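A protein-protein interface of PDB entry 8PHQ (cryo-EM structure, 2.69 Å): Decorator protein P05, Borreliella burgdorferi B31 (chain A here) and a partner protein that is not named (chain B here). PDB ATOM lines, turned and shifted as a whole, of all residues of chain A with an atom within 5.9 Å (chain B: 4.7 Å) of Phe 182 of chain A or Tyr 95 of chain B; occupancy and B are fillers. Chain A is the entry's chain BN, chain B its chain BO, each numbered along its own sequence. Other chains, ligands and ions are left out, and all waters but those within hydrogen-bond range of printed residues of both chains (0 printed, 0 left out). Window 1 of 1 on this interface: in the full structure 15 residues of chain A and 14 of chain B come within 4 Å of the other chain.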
ATOM      1  N   ILE A 118       4.422 -23.893 -17.380  1.00  0.00           N
ATOM      2  CA  ILE A 118       5.226 -23.953 -18.595  1.00  0.00           C
ATOM      3  C   ILE A 118       6.266 -22.841 -18.636  1.00  0.00           C
ATOM      4  O   ILE A 118       7.270 -22.958 -19.347  1.00  0.00           O
ATOM      5  CB  ILE A 118       4.306 -23.910 -19.833  1.00  0.00           C
ATOM      6  CG1 ILE A 118       5.085 -24.261 -21.100  1.00  0.00           C
ATOM      7  CG2 ILE A 118       3.651 -22.545 -19.970  1.00  0.00           C
ATOM      8  CD1 ILE A 118       5.775 -25.598 -21.029  1.00  0.00           C
ATOM      9  N   ASN A 120       8.239 -22.229 -16.300  1.00  0.00           N
ATOM     10  CA  ASN A 120       9.358 -22.728 -15.515  1.00  0.00           C
ATOM     11  C   ASN A 120       9.937 -23.960 -16.200  1.00  0.00           C
ATOM     12  O   ASN A 120       9.193 -24.815 -16.687  1.00  0.00           O
ATOM     13  CB  ASN A 120       8.912 -23.067 -14.091  1.00  0.00           C
ATOM     14  CG  ASN A 120      10.071 -23.188 -13.127  1.00  0.00           C
ATOM     15  OD1 ASN A 120      10.950 -24.033 -13.294  1.00  0.00           O
ATOM     16  ND2 ASN A 120      10.080 -22.340 -12.107  1.00  0.00           N
ATOM     17  N   ASN A 121      11.264 -24.045 -16.243  1.00  0.00           N
ATOM     18  CA  ASN A 121      11.915 -25.143 -16.942  1.00  0.00           C
ATOM     19  C   ASN A 121      11.980 -26.386 -16.061  1.00  0.00           C
ATOM     20  O   ASN A 121      11.985 -26.303 -14.829  1.00  0.00           O
ATOM     21  CB  ASN A 121      13.319 -24.741 -17.395  1.00  0.00           C
ATOM     22  CG  ASN A 121      14.245 -24.447 -16.237  1.00  0.00           C
ATOM     23  OD1 ASN A 121      13.978 -23.564 -15.423  1.00  0.00           O
ATOM     24  ND2 ASN A 121      15.349 -25.178 -16.164  1.00  0.00           N
ATOM     25  N   PHE A 122      12.029 -27.549 -16.709  1.00  0.00           N
ATOM     26  CA  PHE A 122      11.962 -28.825 -16.011  1.00  0.00           C
ATOM     27  C   PHE A 122      12.945 -29.805 -16.635  1.00  0.00           C
ATOM     28  O   PHE A 122      13.189 -29.779 -17.844  1.00  0.00           O
ATOM     29  CB  PHE A 122      10.546 -29.412 -16.066  1.00  0.00           C
ATOM     30  CG  PHE A 122      10.422 -30.767 -15.432  1.00  0.00           C
ATOM     31  CD1 PHE A 122      10.505 -30.911 -14.059  1.00  0.00           C
ATOM     32  CD2 PHE A 122      10.252 -31.899 -16.210  1.00  0.00           C
ATOM     33  CE1 PHE A 122      10.394 -32.154 -13.473  1.00  0.00           C
ATOM     34  CE2 PHE A 122      10.141 -33.144 -15.630  1.00  0.00           C
ATOM     35  CZ  PHE A 122      10.214 -33.272 -14.260  1.00  0.00           C
ATOM     36  N   GLU A 123      13.504 -30.675 -15.796  1.00  0.00           N
ATOM     37  CA  GLU A 123      14.344 -31.783 -16.241  1.00  0.00           C
ATOM     38  C   GLU A 123      13.894 -33.040 -15.516  1.00  0.00           C
ATOM     39  O   GLU A 123      13.910 -33.083 -14.282  1.00  0.00           O
ATOM     40  CB  GLU A 123      15.824 -31.512 -15.964  1.00  0.00           C
ATOM     41  CG  GLU A 123      16.556 -30.802 -17.087  1.00  0.00           C
ATOM     42  CD  GLU A 123      18.057 -30.785 -16.876  1.00  0.00           C
ATOM     43  OE1 GLU A 123      18.517 -31.331 -15.852  1.00  0.00           O
ATOM     44  OE2 GLU A 123      18.776 -30.228 -17.731  1.00  0.00           O
ATOM     45  N   ASN A 160       9.688 -26.127 -27.051  1.00  0.00           N
ATOM     46  CA  ASN A 160      11.027 -26.674 -27.233  1.00  0.00           C
ATOM     47  C   ASN A 160      11.342 -27.645 -26.093  1.00  0.00           C
ATOM     48  O   ASN A 160      11.298 -27.285 -24.914  1.00  0.00           O
ATOM     49  CB  ASN A 160      12.060 -25.553 -27.397  1.00  0.00           C
ATOM     50  CG  ASN A 160      12.111 -24.571 -26.226  1.00  0.00           C
ATOM     51  OD1 ASN A 160      11.888 -24.914 -25.072  1.00  0.00           O
ATOM     52  ND2 ASN A 160      12.423 -23.322 -26.544  1.00  0.00           N
ATOM     53  N   ALA A 161      11.580 -28.904 -26.455  1.00  0.00           N
ATOM     54  CA  ALA A 161      11.926 -29.948 -25.504  1.00  0.00           C
ATOM     55  C   ALA A 161      12.878 -30.920 -26.179  1.00  0.00           C
ATOM     56  O   ALA A 161      12.662 -31.312 -27.329  1.00  0.00           O
ATOM     57  CB  ALA A 161      10.682 -30.688 -24.998  1.00  0.00           C
ATOM     58  N   THR A 162      13.925 -31.311 -25.461  1.00  0.00           N
ATOM     59  CA  THR A 162      14.991 -32.136 -26.013  1.00  0.00           C
ATOM     60  C   THR A 162      15.108 -33.422 -25.209  1.00  0.00           C
ATOM     61  O   THR A 162      15.109 -33.389 -23.974  1.00  0.00           O
ATOM     62  CB  THR A 162      16.323 -31.381 -26.004  1.00  0.00           C
ATOM     63  OG1 THR A 162      16.206 -30.200 -26.808  1.00  0.00           O
ATOM     64  CG2 THR A 162      17.434 -32.251 -26.565  1.00  0.00           C
ATOM     65  N   ALA A 180      14.478 -32.410 -21.040  1.00  0.00           N
ATOM     66  CA  ALA A 180      14.610 -31.052 -20.532  1.00  0.00           C
ATOM     67  C   ALA A 180      13.632 -30.166 -21.292  1.00  0.00           C
ATOM     68  O   ALA A 180      13.700 -30.077 -22.522  1.00  0.00           O
ATOM     69  CB  ALA A 180      16.040 -30.539 -20.693  1.00  0.00           C
ATOM     70  N   VAL A 181      12.728 -29.518 -20.564  1.00  0.00           N
ATOM     71  CA  VAL A 181      11.731 -28.622 -21.139  1.00  0.00           C
ATOM     72  C   VAL A 181      12.067 -27.210 -20.686  1.00  0.00           C
ATOM     73  O   VAL A 181      12.188 -26.953 -19.483  1.00  0.00           O
ATOM     74  CB  VAL A 181      10.306 -29.011 -20.715  1.00  0.00           C
ATOM     75  CG1 VAL A 181       9.290 -28.084 -21.357  1.00  0.00           C
ATOM     76  CG2 VAL A 181      10.020 -30.456 -21.084  1.00  0.00           C
ATOM     77  N   PHE A 182      12.229 -26.296 -21.641  1.00  0.00           N
ATOM     78  CA  PHE A 182      12.649 -24.933 -21.332  1.00  0.00           C
ATOM     79  C   PHE A 182      11.804 -23.916 -22.094  1.00  0.00           C
ATOM     80  O   PHE A 182      12.315 -23.022 -22.771  1.00  0.00           O
ATOM     81  CB  PHE A 182      14.143 -24.740 -21.597  1.00  0.00           C
ATOM     82  CG  PHE A 182      14.636 -25.375 -22.868  1.00  0.00           C
ATOM     83  CD1 PHE A 182      15.064 -26.693 -22.881  1.00  0.00           C
ATOM     84  CD2 PHE A 182      14.730 -24.639 -24.034  1.00  0.00           C
ATOM     85  CE1 PHE A 182      15.532 -27.272 -24.042  1.00  0.00           C
ATOM     86  CE2 PHE A 182      15.200 -25.214 -25.198  1.00  0.00           C
ATOM     87  CZ  PHE A 182      15.601 -26.531 -25.201  1.00  0.00           C
ATOM     88  N   GLY A 183      10.487 -24.047 -21.991  1.00  0.00           N
ATOM     89  CA  GLY A 183       9.579 -22.987 -22.387  1.00  0.00           C
ATOM     90  C   GLY A 183       9.005 -23.155 -23.779  1.00  0.00           C
ATOM     91  O   GLY A 183       9.224 -24.150 -24.477  1.00  0.00           O
ATOM     92  N   ASN A 184       8.242 -22.140 -24.176  1.00  0.00           N
ATOM     93  CA  ASN A 184       7.624 -22.119 -25.493  1.00  0.00           C
ATOM     94  C   ASN A 184       8.658 -21.819 -26.573  1.00  0.00           C
ATOM     95  O   ASN A 184       9.664 -21.147 -26.336  1.00  0.00           O
ATOM     96  CB  ASN A 184       6.507 -21.076 -25.540  1.00  0.00           C
ATOM     97  CG  ASN A 184       5.296 -21.485 -24.727  1.00  0.00           C
ATOM     98  OD1 ASN A 184       5.263 -22.565 -24.141  1.00  0.00           O
ATOM     99  ND2 ASN A 184       4.293 -20.616 -24.682  1.00  0.00           N
ATOM    100  N   GLU B  60      21.894 -22.447 -12.862  1.00  0.00           N
ATOM    101  CA  GLU B  60      22.400 -23.788 -13.101  1.00  0.00           C
ATOM    102  C   GLU B  60      23.884 -23.707 -13.433  1.00  0.00           C
ATOM    103  O   GLU B  60      24.412 -22.632 -13.709  1.00  0.00           O
ATOM    104  CB  GLU B  60      21.634 -24.463 -14.244  1.00  0.00           C
ATOM    105  CG  GLU B  60      20.142 -24.567 -13.989  1.00  0.00           C
ATOM    106  CD  GLU B  60      19.368 -25.025 -15.206  1.00  0.00           C
ATOM    107  OE1 GLU B  60      19.985 -25.196 -16.276  1.00  0.00           O
ATOM    108  OE2 GLU B  60      18.139 -25.214 -15.093  1.00  0.00           O
ATOM    109  N   TYR B  62      26.915 -26.002 -15.772  1.00  0.00           N
ATOM    110  CA  TYR B  62      27.161 -27.073 -16.725  1.00  0.00           C
ATOM    111  C   TYR B  62      28.644 -27.119 -17.043  1.00  0.00           C
ATOM    112  O   TYR B  62      29.349 -26.118 -16.883  1.00  0.00           O
ATOM    113  CB  TYR B  62      26.366 -26.873 -18.023  1.00  0.00           C
ATOM    114  CG  TYR B  62      24.875 -27.085 -17.895  1.00  0.00           C
ATOM    115  CD1 TYR B  62      24.077 -26.158 -17.242  1.00  0.00           C
ATOM    116  CD2 TYR B  62      24.268 -28.211 -18.428  1.00  0.00           C
ATOM    117  CE1 TYR B  62      22.717 -26.347 -17.126  1.00  0.00           C
ATOM    118  CE2 TYR B  62      22.907 -28.409 -18.315  1.00  0.00           C
ATOM    119  CZ  TYR B  62      22.136 -27.472 -17.662  1.00  0.00           C
ATOM    120  OH  TYR B  62      20.779 -27.659 -17.543  1.00  0.00           O
ATOM    121  N   VAL B  73      24.088 -19.685 -24.833  1.00  0.00           N
ATOM    122  CA  VAL B  73      24.593 -21.051 -24.811  1.00  0.00           C
ATOM    123  C   VAL B  73      23.483 -22.011 -25.208  1.00  0.00           C
ATOM    124  O   VAL B  73      22.318 -21.837 -24.826  1.00  0.00           O
ATOM    125  CB  VAL B  73      25.168 -21.428 -23.430  1.00  0.00           C
ATOM    126  CG1 VAL B  73      26.425 -20.636 -23.155  1.00  0.00           C
ATOM    127  CG2 VAL B  73      24.141 -21.191 -22.337  1.00  0.00           C
ATOM    128  N   LYS B  74      23.859 -23.021 -25.989  1.00  0.00           N
ATOM    129  CA  LYS B  74      23.001 -24.120 -26.387  1.00  0.00           C
ATOM    130  C   LYS B  74      23.542 -25.416 -25.800  1.00  0.00           C
ATOM    131  O   LYS B  74      24.703 -25.501 -25.383  1.00  0.00           O
ATOM    132  CB  LYS B  74      22.928 -24.258 -27.911  1.00  0.00           C
ATOM    133  CG  LYS B  74      24.291 -24.318 -28.576  1.00  0.00           C
ATOM    134  CD  LYS B  74      24.178 -24.623 -30.058  1.00  0.00           C
ATOM    135  CE  LYS B  74      25.516 -24.458 -30.758  1.00  0.00           C
ATOM    136  NZ  LYS B  74      25.463 -24.899 -32.180  1.00  0.00           N
ATOM    137  N   LEU B  75      22.683 -26.432 -25.793  1.00  0.00           N
ATOM    138  CA  LEU B  75      23.056 -27.755 -25.317  1.00  0.00           C
ATOM    139  C   LEU B  75      23.764 -28.529 -26.422  1.00  0.00           C
ATOM    140  O   LEU B  75      23.291 -28.574 -27.562  1.00  0.00           O
ATOM    141  CB  LEU B  75      21.816 -28.518 -24.853  1.00  0.00           C
ATOM    142  CG  LEU B  75      21.129 -28.022 -23.580  1.00  0.00           C
ATOM    143  CD1 LEU B  75      20.118 -29.044 -23.087  1.00  0.00           C
ATOM    144  CD2 LEU B  75      22.145 -27.710 -22.499  1.00  0.00           C
ATOM    145  N   ASP B  93      18.343 -23.056 -31.210  1.00  0.00           N
ATOM    146  CA  ASP B  93      18.992 -23.892 -30.209  1.00  0.00           C
ATOM    147  C   ASP B  93      19.294 -23.156 -28.913  1.00  0.00           C
ATOM    148  O   ASP B  93      19.806 -23.782 -27.979  1.00  0.00           O
ATOM    149  CB  ASP B  93      20.287 -24.482 -30.772  1.00  0.00           C
ATOM    150  CG  ASP B  93      20.062 -25.285 -32.035  1.00  0.00           C
ATOM    151  OD1 ASP B  93      19.299 -26.272 -31.985  1.00  0.00           O
ATOM    152  OD2 ASP B  93      20.650 -24.930 -33.079  1.00  0.00           O
ATOM    153  N   LEU B  94      19.004 -21.857 -28.831  1.00  0.00           N
ATOM    154  CA  LEU B  94      19.317 -21.085 -27.634  1.00  0.00           C
ATOM    155  C   LEU B  94      18.677 -21.711 -26.403  1.00  0.00           C
ATOM    156  O   LEU B  94      17.449 -21.802 -26.308  1.00  0.00           O
ATOM    157  CB  LEU B  94      18.844 -19.643 -27.797  1.00  0.00           C
ATOM    158  CG  LEU B  94      19.295 -18.696 -26.686  1.00  0.00           C
ATOM    159  CD1 LEU B  94      20.742 -18.273 -26.885  1.00  0.00           C
ATOM    160  CD2 LEU B  94      18.382 -17.486 -26.605  1.00  0.00           C
ATOM    161  N   TYR B  95      19.514 -22.140 -25.463  1.00  0.00           N
ATOM    162  CA  TYR B  95      19.048 -22.728 -24.214  1.00  0.00           C
ATOM    163  C   TYR B  95      19.141 -21.767 -23.039  1.00  0.00           C
ATOM    164  O   TYR B  95      18.277 -21.792 -22.159  1.00  0.00           O
ATOM    165  CB  TYR B  95      19.844 -23.994 -23.887  1.00  0.00           C
ATOM    166  CG  TYR B  95      19.508 -24.564 -22.530  1.00  0.00           C
ATOM    167  CD1 TYR B  95      18.264 -25.127 -22.282  1.00  0.00           C
ATOM    168  CD2 TYR B  95      20.420 -24.508 -21.485  1.00  0.00           C
ATOM    169  CE1 TYR B  95      17.948 -25.640 -21.041  1.00  0.00           C
ATOM    170  CE2 TYR B  95      20.111 -25.015 -20.240  1.00  0.00           C
ATOM    171  CZ  TYR B  95      18.874 -25.581 -20.023  1.00  0.00           C
ATOM    172  OH  TYR B  95      18.560 -26.089 -18.786  1.00  0.00           O
ATOM    173  N   GLY B  96      20.165 -20.926 -22.999  1.00  0.00           N
ATOM    174  CA  GLY B  96      20.290 -20.018 -21.878  1.00  0.00           C
ATOM    175  C   GLY B  96      21.377 -18.996 -22.110  1.00  0.00           C
ATOM    176  O   GLY B  96      21.879 -18.835 -23.222  1.00  0.00           O
ATOM    177  N   VAL B 110      24.779 -20.823 -15.858  1.00  0.00           N
ATOM    178  CA  VAL B 110      23.811 -20.598 -16.920  1.00  0.00           C
ATOM    179  C   VAL B 110      22.490 -20.175 -16.293  1.00  0.00           C
ATOM    180  O   VAL B 110      22.035 -20.776 -15.309  1.00  0.00           O
ATOM    181  CB  VAL B 110      23.629 -21.855 -17.791  1.00  0.00           C
ATOM    182  CG1 VAL B 110      22.486 -21.666 -18.775  1.00  0.00           C
ATOM    183  CG2 VAL B 110      24.921 -22.190 -18.519  1.00  0.00           C
ATOM    184  N   PRO B 112      18.628 -20.009 -17.385  1.00  0.00           N
ATOM    185  CA  PRO B 112      17.801 -20.558 -18.463  1.00  0.00           C
ATOM    186  C   PRO B 112      17.010 -19.477 -19.179  1.00  0.00           C
ATOM    187  O   PRO B 112      16.760 -18.390 -18.655  1.00  0.00           O
ATOM    188  CB  PRO B 112      16.868 -21.530 -17.733  1.00  0.00           C
ATOM    189  CG  PRO B 112      17.567 -21.846 -16.456  1.00  0.00           C
ATOM    190  CD  PRO B 112      18.284 -20.587 -16.078  1.00  0.00           C
ATOM    191  N   ILE B 113      16.619 -19.801 -20.414  1.00  0.00           N
ATOM    192  CA  ILE B 113      15.868 -18.869 -21.246  1.00  0.00           C
ATOM    193  C   ILE B 113      14.504 -18.554 -20.648  1.00  0.00           C
ATOM    194  O   ILE B 113      13.932 -17.498 -20.935  1.00  0.00           O
ATOM    195  CB  ILE B 113      15.735 -19.433 -22.678  1.00  0.00           C
ATOM    196  CG1 ILE B 113      15.188 -18.369 -23.631  1.00  0.00           C
ATOM    197  CG2 ILE B 113      14.855 -20.672 -22.692  1.00  0.00           C
ATOM    198  CD1 ILE B 113      16.018 -17.109 -23.677  1.00  0.00           C
ATOM    199  N   THR B 114      13.970 -19.441 -19.806  1.00  0.00           N
ATOM    200  CA  THR B 114      12.689 -19.191 -19.158  1.00  0.00           C
ATOM    201  C   THR B 114      12.780 -18.152 -18.050  1.00  0.00           C
ATOM    202  O   THR B 114      11.743 -17.752 -17.514  1.00  0.00           O
ATOM    203  CB  THR B 114      12.118 -20.488 -18.587  1.00  0.00           C
ATOM    204  OG1 THR B 114      13.025 -21.026 -17.615  1.00  0.00           O
ATOM    205  CG2 THR B 114      11.905 -21.504 -19.692  1.00  0.00           C
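The side-chain hydroxyl (OG1) of Thr 114 of chain B is in hydrogen-bond range of the side-chain amide oxygen (OD1) of Asn 121 of chain A, at 3.5 Å. OE2 of Glu 60 of chain B lies within hydrogen-bond range of ND2 of Asn 121 of chain A (3.0 Å). The side-chain hydroxyl of Tyr 62 of chain B sits at hydrogen-bond distance from the side-chain carboxylate of Glu 123 of chain A.
The side-chain hydroxyl (OH) of Tyr 62 of chain B lies within hydrogen-bond range of the side-chain carboxylate (OE1) of Glu 60 of chain B (2.9 Å). The backbone carbonyl oxygen (O) of Tyr 95 of chain B is in hydrogen-bond range of the backbone NH (N) of Ile 113 of chain B. O of Val 73 of chain B sits at hydrogen-bond distance from N of Tyr 95 of chain B, at 2.9 Å. The side-chain amide oxygen of Asn 160 of chain A sits close to the backbone carbonyl oxygen of Phe 182 of chain A, 3.0 Å away. The side-chain hydroxyl of Tyr 95 of chain B lies within hydrogen-bond range of the side-chain carboxylate of Glu 60 of chain B (3.0 Å). The backbone NH of Val 110 of chain B lies within hydrogen-bond range of the backbone carbonyl oxygen of Glu 60 of chain B (2.8 Å).
Tyr 95 of chain B touches Phe 182 of chain A (CE1 to CD1, 3.6 Å). Ile 113 of chain B touches Phe 182 of chain A (CG2 to O, 3.5 Å). C of Phe 182 of chain A touches CG2 of Thr 114 of chain B, at 3.4 Å. Gly 183 of chain A touches Thr 114 of chain B (N to CG2, 3.7 Å).
Of the printed residues of chain B, Glu 123 of chain A touches Tyr 62 (3.3 Å). Of chain B, only Tyr 95 (3.6 Å), Ile 113 (3.5 Å) and Thr 114 (3.4 Å) come within 4 Å of Phe 182 of chain A. Of the printed residues of chain A, Tyr 62 of chain B touches Glu 123. Asp 93 of chain B touches none of the printed residues of chain A. Tyr 95 of chain B touches one residue of chain A. Pro 112 of chain B touches none of the printed residues of chain A. The nearest residue of chain A that does not touch Tyr 95 of chain B is Asn 121 of chain A (4.2 Å). The nearest printed residue of chain A that does not touch Ile 113 of chain B is Asn 160 of chain A (5.3 Å).
Of the 13 printed residues of chain A, 4 touch a printed residue of chain B. Hydrophobic or aromatic side chains of chain A within 4 Å of the printed part of chain B: Phe 182. Hydrophobic or aromatic side chains of chain B that line the printed part of chain A: Tyr 62, Tyr 95 and Ile 113. Among the printed residues, 7 pairs touch across the chains. Among the printed residues, no Asp or Glu carboxylate lies within 4 Å of a Lys or Arg side-chain nitrogen of the other chain.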
